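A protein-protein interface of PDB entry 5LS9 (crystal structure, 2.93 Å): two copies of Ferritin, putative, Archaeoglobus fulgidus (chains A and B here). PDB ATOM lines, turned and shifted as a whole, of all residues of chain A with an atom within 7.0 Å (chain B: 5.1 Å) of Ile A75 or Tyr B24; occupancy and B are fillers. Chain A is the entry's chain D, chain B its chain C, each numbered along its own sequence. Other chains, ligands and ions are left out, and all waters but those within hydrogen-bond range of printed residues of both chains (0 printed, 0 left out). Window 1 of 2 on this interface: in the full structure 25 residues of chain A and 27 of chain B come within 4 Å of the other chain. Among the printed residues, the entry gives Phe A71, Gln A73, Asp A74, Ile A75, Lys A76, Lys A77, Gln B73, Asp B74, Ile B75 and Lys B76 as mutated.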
ATOM      1  N   ILE A  16       7.918 -29.869  26.169  1.00  0.00           N
ATOM      2  CA  ILE A  16       7.644 -28.444  25.985  1.00  0.00           C
ATOM      3  C   ILE A  16       8.161 -28.028  24.609  1.00  0.00           C
ATOM      4  O   ILE A  16       7.426 -27.436  23.807  1.00  0.00           O
ATOM      5  CB  ILE A  16       8.333 -27.595  27.070  1.00  0.00           C
ATOM      6  CG1 ILE A  16       7.592 -27.750  28.399  1.00  0.00           C
ATOM      7  CG2 ILE A  16       8.398 -26.127  26.664  1.00  0.00           C
ATOM      8  CD1 ILE A  16       8.377 -27.277  29.606  1.00  0.00           C
ATOM      9  N   ASN A  17       9.428 -28.361  24.351  1.00  0.00           N
ATOM     10  CA  ASN A  17      10.071 -28.095  23.063  1.00  0.00           C
ATOM     11  C   ASN A  17       9.299 -28.732  21.893  1.00  0.00           C
ATOM     12  O   ASN A  17       9.068 -28.091  20.863  1.00  0.00           O
ATOM     13  CB  ASN A  17      11.526 -28.593  23.085  1.00  0.00           C
ATOM     14  CG  ASN A  17      12.459 -27.722  22.264  1.00  0.00           C
ATOM     15  OD1 ASN A  17      12.676 -26.548  22.589  1.00  0.00           O
ATOM     16  ND2 ASN A  17      13.030 -28.293  21.203  1.00  0.00           N
ATOM     17  N   ALA A  18       8.889 -29.986  22.074  1.00  0.00           N
ATOM     18  CA  ALA A  18       8.116 -30.720  21.066  1.00  0.00           C
ATOM     19  C   ALA A  18       6.739 -30.100  20.828  1.00  0.00           C
ATOM     20  O   ALA A  18       6.265 -30.035  19.691  1.00  0.00           O
ATOM     21  CB  ALA A  18       7.960 -32.178  21.477  1.00  0.00           C
ATOM     22  N   ILE A  20       5.914 -26.958  21.188  1.00  0.00           N
ATOM     23  CA  ILE A  20       6.096 -25.721  20.423  1.00  0.00           C
ATOM     24  C   ILE A  20       6.291 -26.000  18.936  1.00  0.00           C
ATOM     25  O   ILE A  20       5.692 -25.319  18.101  1.00  0.00           O
ATOM     26  CB  ILE A  20       7.262 -24.865  20.954  1.00  0.00           C
ATOM     27  CG1 ILE A  20       6.877 -24.256  22.301  1.00  0.00           C
ATOM     28  CG2 ILE A  20       7.601 -23.750  19.975  1.00  0.00           C
ATOM     29  CD1 ILE A  20       8.039 -23.672  23.073  1.00  0.00           C
ATOM     30  N   TYR A  21       7.120 -26.984  18.597  1.00  0.00           N
ATOM     31  CA  TYR A  21       7.238 -27.400  17.192  1.00  0.00           C
ATOM     32  C   TYR A  21       5.868 -27.888  16.694  1.00  0.00           C
ATOM     33  O   TYR A  21       5.413 -27.499  15.618  1.00  0.00           O
ATOM     34  CB  TYR A  21       8.329 -28.474  16.988  1.00  0.00           C
ATOM     35  CG  TYR A  21       8.380 -29.079  15.584  1.00  0.00           C
ATOM     36  CD1 TYR A  21       8.119 -28.307  14.459  1.00  0.00           C
ATOM     37  CD2 TYR A  21       8.710 -30.421  15.388  1.00  0.00           C
ATOM     38  CE1 TYR A  21       8.161 -28.848  13.187  1.00  0.00           C
ATOM     39  CE2 TYR A  21       8.760 -30.972  14.113  1.00  0.00           C
ATOM     40  CZ  TYR A  21       8.483 -30.174  13.015  1.00  0.00           C
ATOM     41  OH  TYR A  21       8.522 -30.675  11.732  1.00  0.00           O
ATOM     42  N   TYR A  24       4.273 -24.753  15.782  1.00  0.00           N
ATOM     43  CA  TYR A  24       4.909 -24.135  14.601  1.00  0.00           C
ATOM     44  C   TYR A  24       4.540 -24.874  13.311  1.00  0.00           C
ATOM     45  O   TYR A  24       4.275 -24.257  12.288  1.00  0.00           O
ATOM     46  CB  TYR A  24       6.429 -24.126  14.783  1.00  0.00           C
ATOM     47  CG  TYR A  24       7.190 -23.029  14.055  1.00  0.00           C
ATOM     48  CD1 TYR A  24       6.766 -21.705  14.085  1.00  0.00           C
ATOM     49  CD2 TYR A  24       8.387 -23.312  13.411  1.00  0.00           C
ATOM     50  CE1 TYR A  24       7.491 -20.706  13.454  1.00  0.00           C
ATOM     51  CE2 TYR A  24       9.113 -22.325  12.779  1.00  0.00           C
ATOM     52  CZ  TYR A  24       8.661 -21.025  12.799  1.00  0.00           C
ATOM     53  OH  TYR A  24       9.390 -20.058  12.153  1.00  0.00           O
ATOM     54  N   PHE A  71      14.992 -24.602  30.188  1.00  0.00           N
ATOM     55  CA  PHE A  71      15.889 -24.185  29.114  1.00  0.00           C
ATOM     56  C   PHE A  71      15.278 -24.518  27.756  1.00  0.00           C
ATOM     57  O   PHE A  71      14.890 -25.665  27.497  1.00  0.00           O
ATOM     58  CB  PHE A  71      17.249 -24.863  29.254  1.00  0.00           C
ATOM     59  CG  PHE A  71      18.013 -24.443  30.479  1.00  0.00           C
ATOM     60  CD1 PHE A  71      18.277 -23.096  30.729  1.00  0.00           C
ATOM     61  CD2 PHE A  71      18.488 -25.392  31.380  1.00  0.00           C
ATOM     62  CE1 PHE A  71      18.987 -22.701  31.857  1.00  0.00           C
ATOM     63  CE2 PHE A  71      19.204 -25.006  32.508  1.00  0.00           C
ATOM     64  CZ  PHE A  71      19.453 -23.658  32.746  1.00  0.00           C
ATOM     65  N   LEU A  72      15.207 -23.502  26.897  1.00  0.00           N
ATOM     66  CA  LEU A  72      14.576 -23.614  25.582  1.00  0.00           C
ATOM     67  C   LEU A  72      15.610 -23.962  24.509  1.00  0.00           C
ATOM     68  O   LEU A  72      16.685 -23.370  24.462  1.00  0.00           O
ATOM     69  CB  LEU A  72      13.880 -22.292  25.231  1.00  0.00           C
ATOM     70  CG  LEU A  72      12.875 -21.784  26.267  1.00  0.00           C
ATOM     71  CD1 LEU A  72      12.434 -20.371  25.930  1.00  0.00           C
ATOM     72  CD2 LEU A  72      11.672 -22.712  26.359  1.00  0.00           C
ATOM     73  N   GLN A  73      15.281 -24.928  23.656  1.00  0.00           N
ATOM     74  CA  GLN A  73      16.154 -25.294  22.542  1.00  0.00           C
ATOM     75  C   GLN A  73      15.690 -24.592  21.285  1.00  0.00           C
ATOM     76  O   GLN A  73      14.602 -24.020  21.256  1.00  0.00           O
ATOM     77  CB  GLN A  73      16.157 -26.807  22.321  1.00  0.00           C
ATOM     78  CG  GLN A  73      17.243 -27.533  23.093  1.00  0.00           C
ATOM     79  CD  GLN A  73      17.090 -27.396  24.600  1.00  0.00           C
ATOM     80  OE1 GLN A  73      16.018 -27.672  25.153  1.00  0.00           O
ATOM     81  NE2 GLN A  73      18.166 -26.974  25.275  1.00  0.00           N
ATOM     82  N   ASP A  74      16.511 -24.646  20.243  1.00  0.00           N
ATOM     83  CA  ASP A  74      16.163 -24.006  18.986  1.00  0.00           C
ATOM     84  C   ASP A  74      15.054 -24.826  18.319  1.00  0.00           C
ATOM     85  O   ASP A  74      14.831 -25.979  18.692  1.00  0.00           O
ATOM     86  CB  ASP A  74      17.407 -23.814  18.099  1.00  0.00           C
ATOM     87  CG  ASP A  74      17.618 -24.934  17.105  1.00  0.00           C
ATOM     88  OD1 ASP A  74      17.284 -26.095  17.411  1.00  0.00           O
ATOM     89  OD2 ASP A  74      18.150 -24.643  16.012  1.00  0.00           O
ATOM     90  N   ILE A  75      14.355 -24.214  17.364  1.00  0.00           N
ATOM     91  CA  ILE A  75      13.143 -24.775  16.768  1.00  0.00           C
ATOM     92  C   ILE A  75      13.418 -25.090  15.305  1.00  0.00           C
ATOM     93  O   ILE A  75      13.967 -24.251  14.596  1.00  0.00           O
ATOM     94  CB  ILE A  75      11.984 -23.762  16.865  1.00  0.00           C
ATOM     95  CG1 ILE A  75      11.763 -23.334  18.319  1.00  0.00           C
ATOM     96  CG2 ILE A  75      10.704 -24.313  16.250  1.00  0.00           C
ATOM     97  CD1 ILE A  75      11.322 -24.437  19.253  1.00  0.00           C
ATOM     98  N   LYS A  76      13.033 -26.283  14.849  1.00  0.00           N
ATOM     99  CA  LYS A  76      13.365 -26.725  13.483  1.00  0.00           C
ATOM    100  C   LYS A  76      12.400 -26.175  12.435  1.00  0.00           C
ATOM    101  O   LYS A  76      11.273 -25.809  12.747  1.00  0.00           O
ATOM    102  CB  LYS A  76      13.458 -28.259  13.409  1.00  0.00           C
ATOM    103  CG  LYS A  76      14.745 -28.786  14.045  1.00  0.00           C
ATOM    104  CD  LYS A  76      14.763 -30.294  14.273  1.00  0.00           C
ATOM    105  CE  LYS A  76      15.929 -30.758  15.161  1.00  0.00           C
ATOM    106  NZ  LYS A  76      17.301 -30.540  14.602  1.00  0.00           N
ATOM    107  N   LYS A  77      12.856 -26.101  11.191  1.00  0.00           N
ATOM    108  CA  LYS A  77      12.028 -25.588  10.102  1.00  0.00           C
ATOM    109  C   LYS A  77      10.980 -26.634   9.636  1.00  0.00           C
ATOM    110  O   LYS A  77      11.349 -27.686   9.118  1.00  0.00           O
ATOM    111  CB  LYS A  77      12.917 -25.175   8.924  1.00  0.00           C
ATOM    112  CG  LYS A  77      12.153 -24.501   7.791  1.00  0.00           C
ATOM    113  CD  LYS A  77      12.903 -24.492   6.466  1.00  0.00           C
ATOM    114  CE  LYS A  77      12.477 -23.298   5.628  1.00  0.00           C
ATOM    115  NZ  LYS A  77      12.655 -23.482   4.161  1.00  0.00           N
ATOM    116  N   PRO A  78       9.676 -26.333   9.790  1.00  0.00           N
ATOM    117  CA  PRO A  78       8.599 -27.280   9.443  1.00  0.00           C
ATOM    118  C   PRO A  78       8.357 -27.481   7.945  1.00  0.00           C
ATOM    119  O   PRO A  78       8.684 -26.622   7.135  1.00  0.00           O
ATOM    120  CB  PRO A  78       7.354 -26.640  10.068  1.00  0.00           C
ATOM    121  CG  PRO A  78       7.644 -25.185  10.054  1.00  0.00           C
ATOM    122  CD  PRO A  78       9.131 -25.049  10.264  1.00  0.00           C
ATOM    123  N   ILE B  20       9.322 -13.485  15.727  1.00  0.00           N
ATOM    124  CA  ILE B  20       9.053 -14.693  16.517  1.00  0.00           C
ATOM    125  C   ILE B  20      10.232 -15.034  17.459  1.00  0.00           C
ATOM    126  O   ILE B  20      10.029 -15.495  18.588  1.00  0.00           O
ATOM    127  CB  ILE B  20       8.686 -15.890  15.614  1.00  0.00           C
ATOM    128  CG1 ILE B  20       7.288 -15.683  15.034  1.00  0.00           C
ATOM    129  CG2 ILE B  20       8.713 -17.193  16.399  1.00  0.00           C
ATOM    130  CD1 ILE B  20       6.810 -16.798  14.132  1.00  0.00           C
ATOM    131  N   TYR B  21      11.458 -14.795  16.998  1.00  0.00           N
ATOM    132  CA  TYR B  21      12.628 -14.937  17.860  1.00  0.00           C
ATOM    133  C   TYR B  21      12.586 -13.924  19.013  1.00  0.00           C
ATOM    134  O   TYR B  21      13.023 -14.220  20.132  1.00  0.00           O
ATOM    135  CB  TYR B  21      13.932 -14.787  17.073  1.00  0.00           C
ATOM    136  CG  TYR B  21      15.140 -14.720  17.982  1.00  0.00           C
ATOM    137  CD1 TYR B  21      15.565 -15.843  18.685  1.00  0.00           C
ATOM    138  CD2 TYR B  21      15.832 -13.530  18.166  1.00  0.00           C
ATOM    139  CE1 TYR B  21      16.654 -15.791  19.538  1.00  0.00           C
ATOM    140  CE2 TYR B  21      16.925 -13.462  19.016  1.00  0.00           C
ATOM    141  CZ  TYR B  21      17.332 -14.594  19.705  1.00  0.00           C
ATOM    142  OH  TYR B  21      18.420 -14.525  20.561  1.00  0.00           O
ATOM    143  N   SER B  22      12.070 -12.727  18.740  1.00  0.00           N
ATOM    144  CA  SER B  22      11.880 -11.729  19.797  1.00  0.00           C
ATOM    145  C   SER B  22      11.048 -12.359  20.911  1.00  0.00           C
ATOM    146  O   SER B  22      11.442 -12.346  22.067  1.00  0.00           O
ATOM    147  CB  SER B  22      11.178 -10.464  19.279  1.00  0.00           C
ATOM    148  OG  SER B  22      11.639 -10.077  17.997  1.00  0.00           O
ATOM    149  N   ALA B  23       9.909 -12.937  20.538  1.00  0.00           N
ATOM    150  CA  ALA B  23       9.016 -13.558  21.500  1.00  0.00           C
ATOM    151  C   ALA B  23       9.748 -14.655  22.263  1.00  0.00           C
ATOM    152  O   ALA B  23       9.781 -14.645  23.501  1.00  0.00           O
ATOM    153  CB  ALA B  23       7.795 -14.116  20.796  1.00  0.00           C
ATOM    154  N   TYR B  24      10.360 -15.577  21.522  1.00  0.00           N
ATOM    155  CA  TYR B  24      11.064 -16.724  22.120  1.00  0.00           C
ATOM    156  C   TYR B  24      12.165 -16.316  23.116  1.00  0.00           C
ATOM    157  O   TYR B  24      12.413 -17.026  24.087  1.00  0.00           O
ATOM    158  CB  TYR B  24      11.645 -17.609  21.020  1.00  0.00           C
ATOM    159  CG  TYR B  24      11.727 -19.069  21.381  1.00  0.00           C
ATOM    160  CD1 TYR B  24      10.587 -19.776  21.734  1.00  0.00           C
ATOM    161  CD2 TYR B  24      12.941 -19.755  21.342  1.00  0.00           C
ATOM    162  CE1 TYR B  24      10.649 -21.122  22.055  1.00  0.00           C
ATOM    163  CE2 TYR B  24      13.015 -21.102  21.662  1.00  0.00           C
ATOM    164  CZ  TYR B  24      11.865 -21.786  22.017  1.00  0.00           C
ATOM    165  OH  TYR B  24      11.914 -23.129  22.341  1.00  0.00           O
ATOM    166  N   LEU B  25      12.798 -15.170  22.876  1.00  0.00           N
ATOM    167  CA  LEU B  25      13.789 -14.583  23.801  1.00  0.00           C
ATOM    168  C   LEU B  25      13.200 -14.155  25.158  1.00  0.00           C
ATOM    169  O   LEU B  25      13.797 -14.386  26.208  1.00  0.00           O
ATOM    170  CB  LEU B  25      14.461 -13.373  23.130  1.00  0.00           C
ATOM    171  CG  LEU B  25      15.553 -12.593  23.879  1.00  0.00           C
ATOM    172  CD1 LEU B  25      16.766 -13.456  24.200  1.00  0.00           C
ATOM    173  CD2 LEU B  25      15.977 -11.372  23.066  1.00  0.00           C
ATOM    174  N   TYR B  26      12.040 -13.515  25.136  1.00  0.00           N
ATOM    175  CA  TYR B  26      11.423 -13.037  26.374  1.00  0.00           C
ATOM    176  C   TYR B  26      10.865 -14.225  27.146  1.00  0.00           C
ATOM    177  O   TYR B  26      10.967 -14.287  28.369  1.00  0.00           O
ATOM    178  CB  TYR B  26      10.348 -11.975  26.092  1.00  0.00           C
ATOM    179  CG  TYR B  26      10.908 -10.780  25.338  1.00  0.00           C
ATOM    180  CD1 TYR B  26      11.783  -9.892  25.956  1.00  0.00           C
ATOM    181  CD2 TYR B  26      10.581 -10.554  23.998  1.00  0.00           C
ATOM    182  CE1 TYR B  26      12.314  -8.811  25.264  1.00  0.00           C
ATOM    183  CE2 TYR B  26      11.107  -9.476  23.305  1.00  0.00           C
ATOM    184  CZ  TYR B  26      11.976  -8.612  23.940  1.00  0.00           C
ATOM    185  OH  TYR B  26      12.505  -7.549  23.251  1.00  0.00           O
ATOM    186  N   LEU B  27      10.304 -15.191  26.425  1.00  0.00           N
ATOM    187  CA  LEU B  27       9.843 -16.412  27.067  1.00  0.00           C
ATOM    188  C   LEU B  27      10.997 -16.996  27.863  1.00  0.00           C
ATOM    189  O   LEU B  27      10.793 -17.430  28.994  1.00  0.00           O
ATOM    190  CB  LEU B  27       9.321 -17.428  26.047  1.00  0.00           C
ATOM    191  CG  LEU B  27       8.803 -18.756  26.618  1.00  0.00           C
ATOM    192  CD1 LEU B  27       7.750 -18.518  27.695  1.00  0.00           C
ATOM    193  CD2 LEU B  27       8.243 -19.645  25.515  1.00  0.00           C
ATOM    194  N   SER B  28      12.200 -16.985  27.275  1.00  0.00           N
ATOM    195  CA  SER B  28      13.426 -17.429  27.964  1.00  0.00           C
ATOM    196  C   SER B  28      13.775 -16.554  29.166  1.00  0.00           C
ATOM    197  O   SER B  28      14.251 -17.062  30.185  1.00  0.00           O
ATOM    198  CB  SER B  28      14.627 -17.470  27.003  1.00  0.00           C
ATOM    199  OG  SER B  28      15.852 -17.653  27.703  1.00  0.00           O
ATOM    200  N   TRP B  49       6.210 -11.637  25.331  1.00  0.00           N
ATOM    201  CA  TRP B  49       6.182 -12.879  24.521  1.00  0.00           C
ATOM    202  C   TRP B  49       4.915 -12.891  23.693  1.00  0.00           C
ATOM    203  O   TRP B  49       4.980 -12.873  22.466  1.00  0.00           O
ATOM    204  CB  TRP B  49       6.296 -14.118  25.446  1.00  0.00           C
ATOM    205  CG  TRP B  49       5.542 -15.404  25.096  1.00  0.00           C
ATOM    206  CD1 TRP B  49       4.426 -15.887  25.719  1.00  0.00           C
ATOM    207  CD2 TRP B  49       5.920 -16.405  24.139  1.00  0.00           C
ATOM    208  NE1 TRP B  49       4.067 -17.102  25.184  1.00  0.00           N
ATOM    209  CE2 TRP B  49       4.964 -17.434  24.208  1.00  0.00           C
ATOM    210  CE3 TRP B  49       6.964 -16.517  23.213  1.00  0.00           C
ATOM    211  CZ2 TRP B  49       5.015 -18.550  23.387  1.00  0.00           C
ATOM    212  CZ3 TRP B  49       7.017 -17.630  22.394  1.00  0.00           C
ATOM    213  CH2 TRP B  49       6.053 -18.636  22.492  1.00  0.00           C
ATOM    214  N   GLN B  73      10.959 -20.257   8.789  1.00  0.00           N
ATOM    215  CA  GLN B  73      12.323 -20.741   8.970  1.00  0.00           C
ATOM    216  C   GLN B  73      12.562 -21.271  10.374  1.00  0.00           C
ATOM    217  O   GLN B  73      11.670 -21.288  11.224  1.00  0.00           O
ATOM    218  CB  GLN B  73      13.346 -19.625   8.671  1.00  0.00           C
ATOM    219  CG  GLN B  73      13.957 -19.693   7.277  1.00  0.00           C
ATOM    220  CD  GLN B  73      12.944 -19.420   6.179  1.00  0.00           C
ATOM    221  OE1 GLN B  73      12.023 -18.617   6.354  1.00  0.00           O
ATOM    222  NE2 GLN B  73      13.114 -20.081   5.031  1.00  0.00           N
ATOM    223  N   ASP B  74      13.803 -21.701  10.582  1.00  0.00           N
ATOM    224  CA  ASP B  74      14.306 -22.233  11.847  1.00  0.00           C
ATOM    225  C   ASP B  74      14.485 -21.103  12.891  1.00  0.00           C
ATOM    226  O   ASP B  74      14.988 -20.029  12.567  1.00  0.00           O
ATOM    227  CB  ASP B  74      15.592 -23.048  11.504  1.00  0.00           C
ATOM    228  CG  ASP B  74      16.606 -23.130  12.625  1.00  0.00           C
ATOM    229  OD1 ASP B  74      17.077 -22.079  13.107  1.00  0.00           O
ATOM    230  OD2 ASP B  74      17.000 -24.270  12.962  1.00  0.00           O
ATOM    231  N   ILE B  75      14.026 -21.335  14.126  1.00  0.00           N
ATOM    232  CA  ILE B  75      14.204 -20.360  15.215  1.00  0.00           C
ATOM    233  C   ILE B  75      15.432 -20.730  16.021  1.00  0.00           C
ATOM    234  O   ILE B  75      15.554 -21.867  16.457  1.00  0.00           O
ATOM    235  CB  ILE B  75      12.982 -20.290  16.175  1.00  0.00           C
ATOM    236  CG1 ILE B  75      11.926 -19.311  15.661  1.00  0.00           C
ATOM    237  CG2 ILE B  75      13.383 -19.806  17.563  1.00  0.00           C
ATOM    238  CD1 ILE B  75      11.268 -19.731  14.373  1.00  0.00           C
ATOM    239  N   LYS B  76      16.306 -19.752  16.253  1.00  0.00           N
ATOM    240  CA  LYS B  76      17.549 -19.961  17.008  1.00  0.00           C
ATOM    241  C   LYS B  76      17.292 -20.091  18.511  1.00  0.00           C
ATOM    242  O   LYS B  76      16.368 -19.479  19.038  1.00  0.00           O
ATOM    243  CB  LYS B  76      18.519 -18.793  16.783  1.00  0.00           C
ATOM    244  CG  LYS B  76      18.790 -18.414  15.330  1.00  0.00           C
ATOM    245  CD  LYS B  76      19.169 -19.612  14.474  1.00  0.00           C
ATOM    246  CE  LYS B  76      19.767 -19.193  13.137  1.00  0.00           C
ATOM    247  NZ  LYS B  76      20.439 -20.336  12.451  1.00  0.00           N
ATOM    248  N   PRO B  78      17.660 -19.183  22.333  1.00  0.00           N
ATOM    249  CA  PRO B  78      17.955 -17.903  22.962  1.00  0.00           C
ATOM    250  C   PRO B  78      18.918 -18.014  24.126  1.00  0.00           C
ATOM    251  O   PRO B  78      19.023 -19.064  24.768  1.00  0.00           O
ATOM    252  CB  PRO B  78      16.594 -17.463  23.481  1.00  0.00           C
ATOM    253  CG  PRO B  78      15.924 -18.746  23.850  1.00  0.00           C
ATOM    254  CD  PRO B  78      16.460 -19.805  22.923  1.00  0.00           C
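Ile A20 touches Tyr B24, but with the chains exchanged Tyr A24 does not touch Ile B20 (4.02 Å). Tyr A24 touches Ile B75, and with the chains exchanged Ile A75 touches Tyr B24. Asp A74 touches its own counterpart, Asp B74. Ile A75 touches its own counterpart, Ile B75. Positions printed for both chains: 20, 21, 24, 73, 74, 75, 76 and 78.
Of the 14 printed residues of chain A, 8 touch a printed residue of chain B. Printed residues of chain A that touch a printed residue of chain B: Asn A17, Ile A20, Tyr A24, Leu A72, Gln A73, Asp A74, Ile A75 and Lys A77. Hydrophobic or aromatic side chains of chain A that line the printed part of chain B: Ile A20, Tyr A24, Leu A72 and Ile A75. Of the 15 printed residues of chain B, 7 touch a printed residue of chain A. Hydrophobic or aromatic side chains of chain B that line the printed part of chain A: Tyr B24, Ile B75 and Pro B78. Among the printed residues, 16 pairs touch across the chains. Among the printed residues, no Asp or Glu carboxylate lies within 4 Å of a Lys or Arg side-chain nitrogen of the other chain.
The side-chain amino group of Lys B76 is in salt-bridge range of the side-chain carboxylate of Asp B74 (3.8 Å). N of Gln A73 sits at hydrogen-bond distance from OD1 of Asn A17, at 3.2 Å. The backbone carbonyl oxygen (O) of Phe A71 sits close to the side-chain amide oxygen (OE1) of Gln A73 (3.3 Å).
OH of Tyr B24 lies within hydrogen-bond range of O of Gln A73 (3.0 Å). O of Gln B73 sits at hydrogen-bond distance from OH of Tyr A24 (2.8 Å). The backbone carbonyl oxygen (O) of Ile B75 is in hydrogen-bond range of the backbone NH (N) of Ile A75 (2.8 Å). The side-chain carboxylate of Asp A74 lies close to the side-chain carboxylate of Asp B74. The backbone carbonyl oxygen of Ile A75 lies close to the side-chain carboxylate of Asp B74.
Of the printed residues of chain B, Asn A17 touches Tyr B24. Of the printed residues of chain B, Asp A74 touches Asp B74, Ile B75 and Lys B76. Ile A75 touches three residues of chain B. Ile B20 touches none of the printed residues of chain A. Tyr B24 touches just these residues of chain A: Asn A17 (3.5 Å), Ile A20 (3.8 Å), Leu A72 (3.6 Å), Gln A73 (3.0 Å) and Ile A75 (3.4 Å). Leu B25 touches none of the printed residues of chain A. Of the printed residues of chain A, Gln B73 touches Tyr A24 and Lys A77. Of the printed residues of chain A, Ile B75 touches Tyr A24 (2.9 Å), Asp A74 (3.1 Å) and Ile A75 (2.8 Å). Printed residues of chain A within 4 Å of Lys B76: Asp A74 (3.7 Å). The nearest residue of chain B that does not touch Ile A75 is Lys B76 (5.0 Å). The nearest residue of chain A that does not touch Tyr B24 is Asp A74 (5.1 Å).
OD1 of Asn A17 touches OH of Tyr B24, at 3.5 Å. Ile A20 touches Tyr B24 (CD1 to CE1, 3.8 Å). OH of Tyr A24 touches CD1 of Ile B75, 2.9 Å away. Leu A72 touches Tyr B24. Leu A72 touches Ser B28 (CD1 to N, 3.7 Å). Leu A72 touches Pro B78 (O to CD, 3.9 Å). Ile B75 touches Asp A74. Asp A74 touches Lys B76. Tyr B24 touches Ile A75. CB of Lys A77 touches N of Asp B74, at 3.95 Å.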
